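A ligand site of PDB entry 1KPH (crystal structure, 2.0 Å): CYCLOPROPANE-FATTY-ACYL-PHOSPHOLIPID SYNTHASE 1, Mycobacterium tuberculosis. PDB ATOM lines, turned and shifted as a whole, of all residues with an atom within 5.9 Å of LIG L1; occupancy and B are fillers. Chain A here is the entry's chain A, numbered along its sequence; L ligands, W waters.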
ATOM      1  N   PRO A   7      28.926   3.692  18.812  1.00  0.00           N
ATOM      2  CA  PRO A   7      27.539   3.435  18.411  1.00  0.00           C
ATOM      3  C   PRO A   7      26.552   4.055  19.387  1.00  0.00           C
ATOM      4  O   PRO A   7      26.839   4.181  20.580  1.00  0.00           O
ATOM      5  CB  PRO A   7      27.462   1.915  18.404  1.00  0.00           C
ATOM      6  CG  PRO A   7      28.844   1.507  18.017  1.00  0.00           C
ATOM      7  CD  PRO A   7      29.704   2.444  18.837  1.00  0.00           C
ATOM      8  N   HIS A   8      25.379   4.454  18.886  1.00  0.00           N
ATOM      9  CA  HIS A   8      24.362   5.054  19.733  1.00  0.00           C
ATOM     10  C   HIS A   8      23.508   3.964  20.373  1.00  0.00           C
ATOM     11  O   HIS A   8      22.313   3.834  20.085  1.00  0.00           O
ATOM     12  CB  HIS A   8      23.468   5.996  18.920  1.00  0.00           C
ATOM     13  CG  HIS A   8      24.222   7.055  18.165  1.00  0.00           C
ATOM     14  ND1 HIS A   8      24.785   6.837  16.928  1.00  0.00           N
ATOM     15  CD2 HIS A   8      24.510   8.335  18.497  1.00  0.00           C
ATOM     16  CE1 HIS A   8      25.374   7.940  16.519  1.00  0.00           C
ATOM     17  NE2 HIS A   8      25.232   8.865  17.450  1.00  0.00           N
ATOM     18  N   VAL A  12      19.118   3.641  20.097  1.00  0.00           N
ATOM     19  CA  VAL A  12      18.636   2.454  19.393  1.00  0.00           C
ATOM     20  C   VAL A  12      17.960   1.527  20.386  1.00  0.00           C
ATOM     21  O   VAL A  12      16.866   1.030  20.132  1.00  0.00           O
ATOM     22  CB  VAL A  12      19.790   1.726  18.691  1.00  0.00           C
ATOM     23  CG1 VAL A  12      19.302   0.405  18.108  1.00  0.00           C
ATOM     24  CG2 VAL A  12      20.351   2.607  17.587  1.00  0.00           C
ATOM     25  N   TYR A  16      14.118  -0.753  20.450  1.00  0.00           N
ATOM     26  CA  TYR A  16      14.101  -2.214  20.352  1.00  0.00           C
ATOM     27  C   TYR A  16      14.239  -3.029  21.635  1.00  0.00           C
ATOM     28  O   TYR A  16      13.902  -4.212  21.634  1.00  0.00           O
ATOM     29  CB  TYR A  16      15.146  -2.671  19.336  1.00  0.00           C
ATOM     30  CG  TYR A  16      15.016  -1.966  18.000  1.00  0.00           C
ATOM     31  CD1 TYR A  16      15.734  -0.806  17.741  1.00  0.00           C
ATOM     32  CD2 TYR A  16      14.135  -2.432  17.018  1.00  0.00           C
ATOM     33  CE1 TYR A  16      15.596  -0.116  16.534  1.00  0.00           C
ATOM     34  CE2 TYR A  16      13.991  -1.749  15.813  1.00  0.00           C
ATOM     35  CZ  TYR A  16      14.721  -0.597  15.571  1.00  0.00           C
ATOM     36  OH  TYR A  16      14.576   0.078  14.386  1.00  0.00           O
ATOM     37  N   GLN A  31       9.532 -12.188  13.198  1.00  0.00           N
ATOM     38  CA  GLN A  31       9.896 -10.945  13.882  1.00  0.00           C
ATOM     39  C   GLN A  31      10.619  -9.995  12.939  1.00  0.00           C
ATOM     40  O   GLN A  31      11.494  -9.242  13.360  1.00  0.00           O
ATOM     41  CB  GLN A  31      10.788 -11.237  15.102  1.00  0.00           C
ATOM     42  CG  GLN A  31      10.190 -12.216  16.085  1.00  0.00           C
ATOM     43  CD  GLN A  31       8.761 -11.883  16.451  1.00  0.00           C
ATOM     44  OE1 GLN A  31       7.858 -12.707  16.300  1.00  0.00           O
ATOM     45  NE2 GLN A  31       8.541 -10.667  16.942  1.00  0.00           N
ATOM     46  N   THR A  32      10.259 -10.042  11.660  1.00  0.00           N
ATOM     47  CA  THR A  32      10.873  -9.150  10.687  1.00  0.00           C
ATOM     48  C   THR A  32      10.255  -7.769  10.944  1.00  0.00           C
ATOM     49  O   THR A  32       9.037  -7.619  11.002  1.00  0.00           O
ATOM     50  CB  THR A  32      10.603  -9.610   9.242  1.00  0.00           C
ATOM     51  OG1 THR A  32      11.215 -10.886   9.026  1.00  0.00           O
ATOM     52  CG2 THR A  32      11.165  -8.614   8.241  1.00  0.00           C
ATOM     53  N   TYR A  33      11.120  -6.765  11.079  1.00  0.00           N
ATOM     54  CA  TYR A  33      10.657  -5.415  11.377  1.00  0.00           C
ATOM     55  C   TYR A  33      11.111  -4.452  10.283  1.00  0.00           C
ATOM     56  O   TYR A  33      11.966  -3.587  10.507  1.00  0.00           O
ATOM     57  CB  TYR A  33      11.232  -5.021  12.755  1.00  0.00           C
ATOM     58  CG  TYR A  33      10.578  -3.855  13.465  1.00  0.00           C
ATOM     59  CD1 TYR A  33       9.375  -3.295  13.017  1.00  0.00           C
ATOM     60  CD2 TYR A  33      11.154  -3.322  14.619  1.00  0.00           C
ATOM     61  CE1 TYR A  33       8.766  -2.243  13.693  1.00  0.00           C
ATOM     62  CE2 TYR A  33      10.555  -2.263  15.303  1.00  0.00           C
ATOM     63  CZ  TYR A  33       9.368  -1.724  14.837  1.00  0.00           C
ATOM     64  OH  TYR A  33       8.775  -0.673  15.518  1.00  0.00           O
ATOM     65  N   SER A  34      10.522  -4.615   9.106  1.00  0.00           N
ATOM     66  CA  SER A  34      10.834  -3.804   7.934  1.00  0.00           C
ATOM     67  C   SER A  34       9.765  -4.073   6.872  1.00  0.00           C
ATOM     68  O   SER A  34       8.953  -4.975   7.034  1.00  0.00           O
ATOM     69  CB  SER A  34      12.220  -4.154   7.402  1.00  0.00           C
ATOM     70  OG  SER A  34      12.382  -5.564   7.256  1.00  0.00           O
ATOM     71  N   LYS A  52      10.361 -10.650   0.827  1.00  0.00           N
ATOM     72  CA  LYS A  52      11.207  -9.472   0.896  1.00  0.00           C
ATOM     73  C   LYS A  52      12.639  -9.940   1.155  1.00  0.00           C
ATOM     74  O   LYS A  52      13.582  -9.463   0.516  1.00  0.00           O
ATOM     75  CB  LYS A  52      10.740  -8.529   2.013  1.00  0.00           C
ATOM     76  CG  LYS A  52      11.640  -7.307   2.279  1.00  0.00           C
ATOM     77  CD  LYS A  52      12.790  -7.631   3.228  1.00  0.00           C
ATOM     78  CE  LYS A  52      12.291  -8.048   4.610  1.00  0.00           C
ATOM     79  NZ  LYS A  52      11.367  -7.042   5.221  1.00  0.00           N
ATOM     80  N   ASP A  70      25.140  -9.212   8.192  1.00  0.00           N
ATOM     81  CA  ASP A  70      23.847  -8.544   8.281  1.00  0.00           C
ATOM     82  C   ASP A  70      23.978  -7.400   9.271  1.00  0.00           C
ATOM     83  O   ASP A  70      23.989  -7.625  10.491  1.00  0.00           O
ATOM     84  CB  ASP A  70      22.756  -9.508   8.766  1.00  0.00           C
ATOM     85  CG  ASP A  70      21.384  -8.855   8.818  1.00  0.00           C
ATOM     86  OD1 ASP A  70      21.306  -7.606   8.849  1.00  0.00           O
ATOM     87  OD2 ASP A  70      20.370  -9.591   8.838  1.00  0.00           O
ATOM     88  N   VAL A  71      24.085  -6.185   8.759  1.00  0.00           N
ATOM     89  CA  VAL A  71      24.209  -4.990   9.597  1.00  0.00           C
ATOM     90  C   VAL A  71      22.840  -4.561  10.108  1.00  0.00           C
ATOM     91  O   VAL A  71      22.013  -4.064   9.346  1.00  0.00           O
ATOM     92  CB  VAL A  71      24.847  -3.825   8.804  1.00  0.00           C
ATOM     93  CG1 VAL A  71      25.008  -2.606   9.704  1.00  0.00           C
ATOM     94  CG2 VAL A  71      26.200  -4.258   8.266  1.00  0.00           C
ATOM     95  N   GLY A  72      22.615  -4.759  11.400  1.00  0.00           N
ATOM     96  CA  GLY A  72      21.327  -4.423  11.982  1.00  0.00           C
ATOM     97  C   GLY A  72      20.425  -5.612  11.773  1.00  0.00           C
ATOM     98  O   GLY A  72      19.303  -5.492  11.287  1.00  0.00           O
ATOM     99  N   CYS A  73      20.938  -6.783  12.149  1.00  0.00           N
ATOM    100  CA  CYS A  73      20.251  -8.076  11.985  1.00  0.00           C
ATOM    101  C   CYS A  73      18.865  -8.221  12.620  1.00  0.00           C
ATOM    102  O   CYS A  73      18.155  -9.165  12.320  1.00  0.00           O
ATOM    103  CB  CYS A  73      21.152  -9.194  12.508  1.00  0.00           C
ATOM    104  SG  CYS A  73      21.387  -9.221  14.322  1.00  0.00           S
ATOM    105  N   GLY A  74      18.490  -7.290  13.504  1.00  0.00           N
ATOM    106  CA  GLY A  74      17.189  -7.389  14.144  1.00  0.00           C
ATOM    107  C   GLY A  74      17.056  -8.675  14.935  1.00  0.00           C
ATOM    108  O   GLY A  74      17.972  -9.054  15.665  1.00  0.00           O
ATOM    109  N   TRP A  75      15.923  -9.342  14.821  1.00  0.00           N
ATOM    110  CA  TRP A  75      15.722 -10.593  15.543  1.00  0.00           C
ATOM    111  C   TRP A  75      16.194 -11.816  14.743  1.00  0.00           C
ATOM    112  O   TRP A  75      15.795 -12.948  15.011  1.00  0.00           O
ATOM    113  CB  TRP A  75      14.248 -10.722  15.965  1.00  0.00           C
ATOM    114  CG  TRP A  75      13.947  -9.862  17.179  1.00  0.00           C
ATOM    115  CD1 TRP A  75      14.293 -10.128  18.482  1.00  0.00           C
ATOM    116  CD2 TRP A  75      13.317  -8.580  17.190  1.00  0.00           C
ATOM    117  NE1 TRP A  75      13.920  -9.087  19.299  1.00  0.00           N
ATOM    118  CE2 TRP A  75      13.321  -8.124  18.535  1.00  0.00           C
ATOM    119  CE3 TRP A  75      12.756  -7.763  16.200  1.00  0.00           C
ATOM    120  CZ2 TRP A  75      12.776  -6.888  18.905  1.00  0.00           C
ATOM    121  CZ3 TRP A  75      12.218  -6.533  16.568  1.00  0.00           C
ATOM    122  CH2 TRP A  75      12.237  -6.107  17.917  1.00  0.00           C
ATOM    123  N   THR A  78      16.514 -12.807   8.777  1.00  0.00           N
ATOM    124  CA  THR A  78      17.282 -12.765   7.552  1.00  0.00           C
ATOM    125  C   THR A  78      18.520 -13.653   7.625  1.00  0.00           C
ATOM    126  O   THR A  78      18.804 -14.406   6.680  1.00  0.00           O
ATOM    127  CB  THR A  78      17.676 -11.316   7.202  1.00  0.00           C
ATOM    128  OG1 THR A  78      16.493 -10.586   6.865  1.00  0.00           O
ATOM    129  CG2 THR A  78      18.644 -11.278   6.014  1.00  0.00           C
ATOM    130  N   LEU A  93      24.934  -8.055  13.241  1.00  0.00           N
ATOM    131  CA  LEU A  93      25.252  -6.973  14.173  1.00  0.00           C
ATOM    132  C   LEU A  93      23.996  -6.255  14.623  1.00  0.00           C
ATOM    133  O   LEU A  93      23.081  -6.022  13.841  1.00  0.00           O
ATOM    134  CB  LEU A  93      26.193  -5.969  13.487  1.00  0.00           C
ATOM    135  CG  LEU A  93      27.501  -6.512  12.915  1.00  0.00           C
ATOM    136  CD1 LEU A  93      28.246  -5.397  12.177  1.00  0.00           C
ATOM    137  CD2 LEU A  93      28.348  -7.088  14.046  1.00  0.00           C
ATOM    138  N   THR A  94      23.936  -5.907  15.919  1.00  0.00           N
ATOM    139  CA  THR A  94      22.788  -5.200  16.469  1.00  0.00           C
ATOM    140  C   THR A  94      23.143  -4.510  17.796  1.00  0.00           C
ATOM    141  O   THR A  94      23.932  -5.035  18.579  1.00  0.00           O
ATOM    142  CB  THR A  94      21.600  -6.141  16.736  1.00  0.00           C
ATOM    143  OG1 THR A  94      20.499  -5.390  17.241  1.00  0.00           O
ATOM    144  CG2 THR A  94      21.976  -7.208  17.771  1.00  0.00           C
ATOM    145  N   LEU A  95      22.542  -3.356  18.031  1.00  0.00           N
ATOM    146  CA  LEU A  95      22.804  -2.599  19.256  1.00  0.00           C
ATOM    147  C   LEU A  95      21.769  -2.954  20.317  1.00  0.00           C
ATOM    148  O   LEU A  95      21.843  -2.453  21.451  1.00  0.00           O
ATOM    149  CB  LEU A  95      22.749  -1.099  18.969  1.00  0.00           C
ATOM    150  CG  LEU A  95      23.596  -0.617  17.790  1.00  0.00           C
ATOM    151  CD1 LEU A  95      23.528   0.909  17.700  1.00  0.00           C
ATOM    152  CD2 LEU A  95      25.043  -1.080  17.960  1.00  0.00           C
ATOM    153  N   SER A  96      20.817  -3.799  19.958  1.00  0.00           N
ATOM    154  CA  SER A  96      19.751  -4.207  20.867  1.00  0.00           C
ATOM    155  C   SER A  96      20.145  -5.400  21.728  1.00  0.00           C
ATOM    156  O   SER A  96      20.458  -6.484  21.215  1.00  0.00           O
ATOM    157  CB  SER A  96      18.494  -4.546  20.066  1.00  0.00           C
ATOM    158  OG  SER A  96      17.450  -4.994  20.912  1.00  0.00           O
ATOM    159  N   GLN A  99      17.718  -8.288  21.274  1.00  0.00           N
ATOM    160  CA  GLN A  99      17.843  -8.922  19.967  1.00  0.00           C
ATOM    161  C   GLN A  99      19.089  -9.798  19.954  1.00  0.00           C
ATOM    162  O   GLN A  99      19.066 -10.909  19.427  1.00  0.00           O
ATOM    163  CB  GLN A  99      17.921  -7.870  18.860  1.00  0.00           C
ATOM    164  CG  GLN A  99      16.662  -7.021  18.728  1.00  0.00           C
ATOM    165  CD  GLN A  99      16.711  -6.097  17.526  1.00  0.00           C
ATOM    166  OE1 GLN A  99      17.776  -5.633  17.131  1.00  0.00           O
ATOM    167  NE2 GLN A  99      15.547  -5.815  16.950  1.00  0.00           N
ATOM    168  N   ALA A 121      27.146  -5.194  18.885  1.00  0.00           N
ATOM    169  CA  ALA A 121      28.060  -4.127  18.488  1.00  0.00           C
ATOM    170  C   ALA A 121      27.581  -3.474  17.205  1.00  0.00           C
ATOM    171  O   ALA A 121      26.744  -4.028  16.488  1.00  0.00           O
ATOM    172  CB  ALA A 121      29.454  -4.702  18.276  1.00  0.00           C
ATOM    173  N   GLY A 122      28.093  -2.289  16.912  1.00  0.00           N
ATOM    174  CA  GLY A 122      27.703  -1.588  15.708  1.00  0.00           C
ATOM    175  C   GLY A 122      28.749  -1.800  14.635  1.00  0.00           C
ATOM    176  O   GLY A 122      29.865  -2.242  14.930  1.00  0.00           O
ATOM    177  N   TRP A 123      28.421  -1.496  13.381  1.00  0.00           N
ATOM    178  CA  TRP A 123      29.392  -1.662  12.304  1.00  0.00           C
ATOM    179  C   TRP A 123      30.603  -0.798  12.629  1.00  0.00           C
ATOM    180  O   TRP A 123      31.695  -1.022  12.101  1.00  0.00           O
ATOM    181  CB  TRP A 123      28.811  -1.228  10.956  1.00  0.00           C
ATOM    182  CG  TRP A 123      28.184   0.139  10.972  1.00  0.00           C
ATOM    183  CD1 TRP A 123      26.868   0.438  11.212  1.00  0.00           C
ATOM    184  CD2 TRP A 123      28.842   1.384  10.750  1.00  0.00           C
ATOM    185  NE1 TRP A 123      26.678   1.790  11.151  1.00  0.00           N
ATOM    186  CE2 TRP A 123      27.875   2.398  10.868  1.00  0.00           C
ATOM    187  CE3 TRP A 123      30.165   1.746  10.460  1.00  0.00           C
ATOM    188  CZ2 TRP A 123      28.183   3.755  10.711  1.00  0.00           C
ATOM    189  CZ3 TRP A 123      30.479   3.095  10.300  1.00  0.00           C
ATOM    190  CH2 TRP A 123      29.485   4.082  10.425  1.00  0.00           C
ATOM    191  N   GLU A 124      30.410   0.189  13.496  1.00  0.00           N
ATOM    192  CA  GLU A 124      31.478   1.091  13.904  1.00  0.00           C
ATOM    193  C   GLU A 124      32.561   0.348  14.667  1.00  0.00           C
ATOM    194  O   GLU A 124      33.689   0.831  14.780  1.00  0.00           O
ATOM    195  CB  GLU A 124      30.931   2.213  14.797  1.00  0.00           C
ATOM    196  CG  GLU A 124      29.920   3.165  14.163  1.00  0.00           C
ATOM    197  CD  GLU A 124      28.475   2.723  14.341  1.00  0.00           C
ATOM    198  OE1 GLU A 124      27.579   3.587  14.286  1.00  0.00           O
ATOM    199  OE2 GLU A 124      28.236   1.510  14.538  1.00  0.00           O
ATOM    200  N   SER A 135      21.754  -5.039   4.565  1.00  0.00           N
ATOM    201  CA  SER A 135      21.355  -4.168   5.665  1.00  0.00           C
ATOM    202  C   SER A 135      19.957  -3.678   5.353  1.00  0.00           C
ATOM    203  O   SER A 135      19.743  -2.947   4.376  1.00  0.00           O
ATOM    204  CB  SER A 135      22.317  -2.994   5.832  1.00  0.00           C
ATOM    205  OG  SER A 135      21.994  -2.258   6.991  1.00  0.00           O
ATOM    206  N   ILE A 136      19.015  -4.087   6.187  1.00  0.00           N
ATOM    207  CA  ILE A 136      17.619  -3.710   5.994  1.00  0.00           C
ATOM    208  C   ILE A 136      17.069  -2.901   7.162  1.00  0.00           C
ATOM    209  O   ILE A 136      16.982  -3.400   8.290  1.00  0.00           O
ATOM    210  CB  ILE A 136      16.750  -4.973   5.800  1.00  0.00           C
ATOM    211  CG1 ILE A 136      17.235  -5.747   4.571  1.00  0.00           C
ATOM    212  CG2 ILE A 136      15.287  -4.588   5.651  1.00  0.00           C
ATOM    213  CD1 ILE A 136      16.775  -7.184   4.510  1.00  0.00           C
ATOM    214  N   GLY A 137      16.696  -1.657   6.881  1.00  0.00           N
ATOM    215  CA  GLY A 137      16.122  -0.803   7.912  1.00  0.00           C
ATOM    216  C   GLY A 137      17.014  -0.440   9.084  1.00  0.00           C
ATOM    217  O   GLY A 137      16.521  -0.175  10.173  1.00  0.00           O
ATOM    218  N   ALA A 138      18.325  -0.422   8.868  1.00  0.00           N
ATOM    219  CA  ALA A 138      19.257  -0.056   9.941  1.00  0.00           C
ATOM    220  C   ALA A 138      19.858   1.311   9.632  1.00  0.00           C
ATOM    221  O   ALA A 138      20.173   2.097  10.533  1.00  0.00           O
ATOM    222  CB  ALA A 138      20.364  -1.103  10.059  1.00  0.00           C
ATOM    223  N   HIS A 141      19.135   4.618  11.270  1.00  0.00           N
ATOM    224  CA  HIS A 141      19.642   4.839  12.617  1.00  0.00           C
ATOM    225  C   HIS A 141      21.076   5.349  12.638  1.00  0.00           C
ATOM    226  O   HIS A 141      21.569   5.793  13.687  1.00  0.00           O
ATOM    227  CB  HIS A 141      19.588   3.534  13.422  1.00  0.00           C
ATOM    228  CG  HIS A 141      18.206   3.145  13.868  1.00  0.00           C
ATOM    229  ND1 HIS A 141      17.517   3.851  14.833  1.00  0.00           N
ATOM    230  CD2 HIS A 141      17.403   2.130  13.499  1.00  0.00           C
ATOM    231  CE1 HIS A 141      16.349   3.281  15.045  1.00  0.00           C
ATOM    232  NE2 HIS A 141      16.248   2.231  14.242  1.00  0.00           N
ATOM    233  N   PHE A 142      21.749   5.291  11.491  1.00  0.00           N
ATOM    234  CA  PHE A 142      23.143   5.710  11.403  1.00  0.00           C
ATOM    235  C   PHE A 142      23.356   7.217  11.544  1.00  0.00           C
ATOM    236  O   PHE A 142      24.301   7.648  12.214  1.00  0.00           O
ATOM    237  CB  PHE A 142      23.753   5.255  10.059  1.00  0.00           C
ATOM    238  CG  PHE A 142      23.755   3.749   9.867  1.00  0.00           C
ATOM    239  CD1 PHE A 142      23.305   2.883  10.860  1.00  0.00           C
ATOM    240  CD2 PHE A 142      24.227   3.214   8.671  1.00  0.00           C
ATOM    241  CE1 PHE A 142      23.332   1.497  10.667  1.00  0.00           C
ATOM    242  CE2 PHE A 142      24.250   1.828   8.469  1.00  0.00           C
ATOM    243  CZ  PHE A 142      23.804   0.976   9.472  1.00  0.00           C
ATOM    244  N   ARG A 146      27.236   9.830   9.678  1.00  0.00           N
ATOM    245  CA  ARG A 146      28.037   8.616   9.592  1.00  0.00           C
ATOM    246  C   ARG A 146      27.878   7.824   8.298  1.00  0.00           C
ATOM    247  O   ARG A 146      28.514   6.784   8.132  1.00  0.00           O
ATOM    248  CB  ARG A 146      27.755   7.711  10.790  1.00  0.00           C
ATOM    249  CG  ARG A 146      28.120   8.335  12.129  1.00  0.00           C
ATOM    250  CD  ARG A 146      28.066   7.324  13.262  1.00  0.00           C
ATOM    251  NE  ARG A 146      28.365   7.955  14.540  1.00  0.00           N
ATOM    252  CZ  ARG A 146      28.406   7.321  15.699  1.00  0.00           C
ATOM    253  NH1 ARG A 146      28.170   6.009  15.761  1.00  0.00           N
ATOM    254  NH2 ARG A 146      28.681   7.990  16.818  1.00  0.00           N
HETATM  255  N1  LIG L   1      17.071  -5.827   9.655  1.00  0.00           N
HETATM  256  C1  LIG L   1      16.075  -6.311  10.598  1.00  0.00           C
HETATM  257  C2  LIG L   1      15.854  -5.303  11.752  1.00  0.00           C
HETATM  258  C3  LIG L   1      15.616  -3.820  11.410  1.00  0.00           C
HETATM  259  C4  LIG L   1      14.733  -6.581   9.895  1.00  0.00           C
HETATM  260  O1  LIG L   1      13.832  -7.159  10.534  1.00  0.00           O
HETATM  261  C5  LIG L   1      16.918  -1.835  12.917  1.00  0.00           C
HETATM  262  C6  LIG L   1      18.093  -2.731  13.308  1.00  0.00           C
HETATM  263  O2  LIG L   1      19.376  -2.152  12.973  1.00  0.00           O
HETATM  264  C7  LIG L   1      18.135  -3.044  14.797  1.00  0.00           C
HETATM  265  O3  LIG L   1      18.418  -4.456  14.981  1.00  0.00           O
HETATM  266  C8  LIG L   1      19.248  -2.158  15.315  1.00  0.00           C
HETATM  267  O4  LIG L   1      19.824  -2.669  16.523  1.00  0.00           O
HETATM  268  C9  LIG L   1      20.198  -2.149  14.164  1.00  0.00           C
HETATM  269  N2  LIG L   1      21.123  -1.007  14.182  1.00  0.00           N
HETATM  270  C10 LIG L   1      20.891   0.322  14.303  1.00  0.00           C
HETATM  271  N3  LIG L   1      21.924   1.108  14.270  1.00  0.00           N
HETATM  272  C11 LIG L   1      22.962   0.199  14.114  1.00  0.00           C
HETATM  273  C12 LIG L   1      24.494   0.337  13.990  1.00  0.00           C
HETATM  274  N4  LIG L   1      25.131   1.527  14.015  1.00  0.00           N
HETATM  275  N5  LIG L   1      25.214  -0.827  13.840  1.00  0.00           N
HETATM  276  C13 LIG L   1      24.561  -2.016  13.810  1.00  0.00           C
HETATM  277  N6  LIG L   1      23.231  -2.268  13.899  1.00  0.00           N
HETATM  278  C14 LIG L   1      22.484  -1.102  14.058  1.00  0.00           C
HETATM  279  C1  LG2 L   2      12.510  12.214   9.698  1.00  0.00           C
HETATM  280  C2  LG2 L   2      13.068  11.353  10.833  1.00  0.00           C
HETATM  281  C3  LG2 L   2      12.984   9.868  10.459  1.00  0.00           C
HETATM  282  C4  LG2 L   2      13.490   8.879  11.519  1.00  0.00           C
HETATM  283  C5  LG2 L   2      13.308   7.466  10.940  1.00  0.00           C
HETATM  284  C6  LG2 L   2      13.700   6.312  11.878  1.00  0.00           C
HETATM  285  C7  LG2 L   2      13.366   5.038  11.086  1.00  0.00           C
HETATM  286  C8  LG2 L   2      13.522   3.732  11.872  1.00  0.00           C
HETATM  287  C9  LG2 L   2      13.087   2.570  10.953  1.00  0.00           C
HETATM  288  C10 LG2 L   2      13.013   1.267  11.744  1.00  0.00           C
HETATM  289  N1  LG2 L   2      12.397  -0.013  11.154  1.00  0.00           N
HETATM  290  C11 LG2 L   2      12.420  -1.034  12.271  1.00  0.00           C
HETATM  291  C12 LG2 L   2      13.247  -0.576  10.038  1.00  0.00           C
HETATM  292  C13 LG2 L   2      10.971   0.103  10.592  1.00  0.00           C
HETATM  293  C14 LG2 L   2       9.774   0.633  11.422  1.00  0.00           C
HETATM  294  C15 LG2 L   2       8.496   1.031  10.638  1.00  0.00           C
HETATM  295  C16 LG2 L   2       8.585   2.178   9.598  1.00  0.00           C
HETATM  296  C17 LG2 L   2       8.881   3.547  10.230  1.00  0.00           C
HETATM  297  C18 LG2 L   2       8.926   4.681   9.193  1.00  0.00           C
HETATM  298  C19 LG2 L   2       9.221   6.025   9.887  1.00  0.00           C
HETATM  299  C20 LG2 L   2       9.209   7.155   8.838  1.00  0.00           C
HETATM  300  C21 LG2 L   2       9.455   8.519   9.476  1.00  0.00           C
HETATM  301  C22 LG2 L   2       9.404   9.589   8.383  1.00  0.00           C
HETATM  302  O   HOH W   1      17.957  -8.441   8.550  1.00  0.00           O
HETATM  303  O   HOH W   2      25.318   3.804  16.370  1.00  0.00           O
HETATM  304  O   HOH W   3      23.067   3.515  14.939  1.00  0.00           O
HETATM  305  O   HOH W   4      13.967  -8.240  12.890  1.00  0.00           O
HETATM  306  O   HOH W   5      19.791  -5.497   8.343  1.00  0.00           O
HETATM  307  O   HOH W   6      14.570  -8.337   6.944  1.00  0.00           O
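Water W4 lies within hydrogen-bond range of O1 of LIG L1 (2.6 Å), O of Gln 31 (2.7 Å) and N of Trp 75 (3.0 Å). Water W3 lies within hydrogen-bond range of N3 of LIG L1 (2.7 Å) and O of His 141 (3.0 Å). Water W1 lies within hydrogen-bond range of OD2 of Asp 70 (2.7 Å), N1 of LIG L1 (3.0 Å) and OG1 of Thr 78 (3.1 Å). Water W2 lies within hydrogen-bond range of N of His 8 (2.6 Å), OE1 of Glu 124 (3.1 Å) and N4 of LIG L1 (3.3 Å).
An oxygen (O3) of LIG L1 is in hydrogen-bond range of the side-chain amide oxygen (OE1) of Gln 99 (2.5 Å). A nitrogen (N1) of LIG L1 sits at hydrogen-bond distance from the backbone carbonyl oxygen of Gly 72 (2.8 Å). The backbone carbonyl oxygen (O) of Ile 136 sits at hydrogen-bond distance from a nitrogen (N1) of LIG L1 (2.8 Å). An oxygen (O1) of LIG L1 lies within hydrogen-bond range of the backbone NH (N) of Tyr 33. O4 of LIG L1 lies within hydrogen-bond range of OG1 of Thr 94, at 2.9 Å. OE2 of Glu 124 lies within hydrogen-bond range of N4 of LIG L1 (3.1 Å). An oxygen (O4) of LIG L1 is in hydrogen-bond range of the backbone NH of Leu 95 (3.2 Å). O3 of LIG L1 lies within hydrogen-bond range of N of Gly 74 (3.2 Å). The backbone NH of Trp 123 lies within hydrogen-bond range of a nitrogen (N5) of LIG L1, 3.3 Å away.
Val 12 touches LIG L1 (CG1 to O4, 3.5 Å). Tyr 16 touches LIG L1 (OH to C5, 3.4 Å). Thr 32 touches LIG L1 (CA to O1, 3.6 Å). OG of Ser 34 touches C4 of LIG L1, at 3.7 Å. Cys 73 touches LIG L1. O of Leu 93 touches N6 of LIG L1 (3.8 Å). Ser 96 touches LIG L1. O of Ala 121 touches C13 of LIG L1 (3.998 Å). CA of Gly 122 touches N5 of LIG L1, at 3.2 Å. Gly 137 touches LIG L1 (O to C5, 3.2 Å). CB of Ala 138 touches O2 of LIG L1, 3.3 Å away. CB of His 141 touches N3 of LIG L1, at 3.5 Å. CE1 of Phe 142 touches C11 of LIG L1 (3.7 Å). 22 residues have an atom within 4 Å of LIG L1: Val 12, Tyr 16, Thr 32, Tyr 33, Ser 34, Gly 72, Cys 73, Gly 74, Leu 93, Thr 94, Leu 95, Ser 96, Gln 99, Ala 121, Gly 122, Trp 123, Glu 124, Ile 136, Gly 137, Ala 138, His 141 and Phe 142.
OE1 of Gln 99 is in hydrogen-bond range of OG1 of Thr 94, at 2.7 Å. The backbone NH of Gln 99 lies close to the side-chain hydroxyl of Ser 96, at 3.3 Å. The backbone NH (N) of Gly 72 lies within hydrogen-bond range of the backbone carbonyl oxygen (O) of Leu 93 (2.8 Å). The backbone carbonyl oxygen of Thr 94 lies within hydrogen-bond range of the backbone NH of Ala 121, 3.2 Å away. The side-chain carboxylate (OE1) of Glu 124 lies within salt-bridge range of the guanidinium group (NH1) of Arg 146. OG of Ser 34 sits at hydrogen-bond distance from NZ of Lys 52 (2.7 Å). N of Cys 73 is in hydrogen-bond range of O of Leu 93, at 2.8 Å. N of Leu 93 lies within hydrogen-bond range of O of Asp 70, 2.9 Å away.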
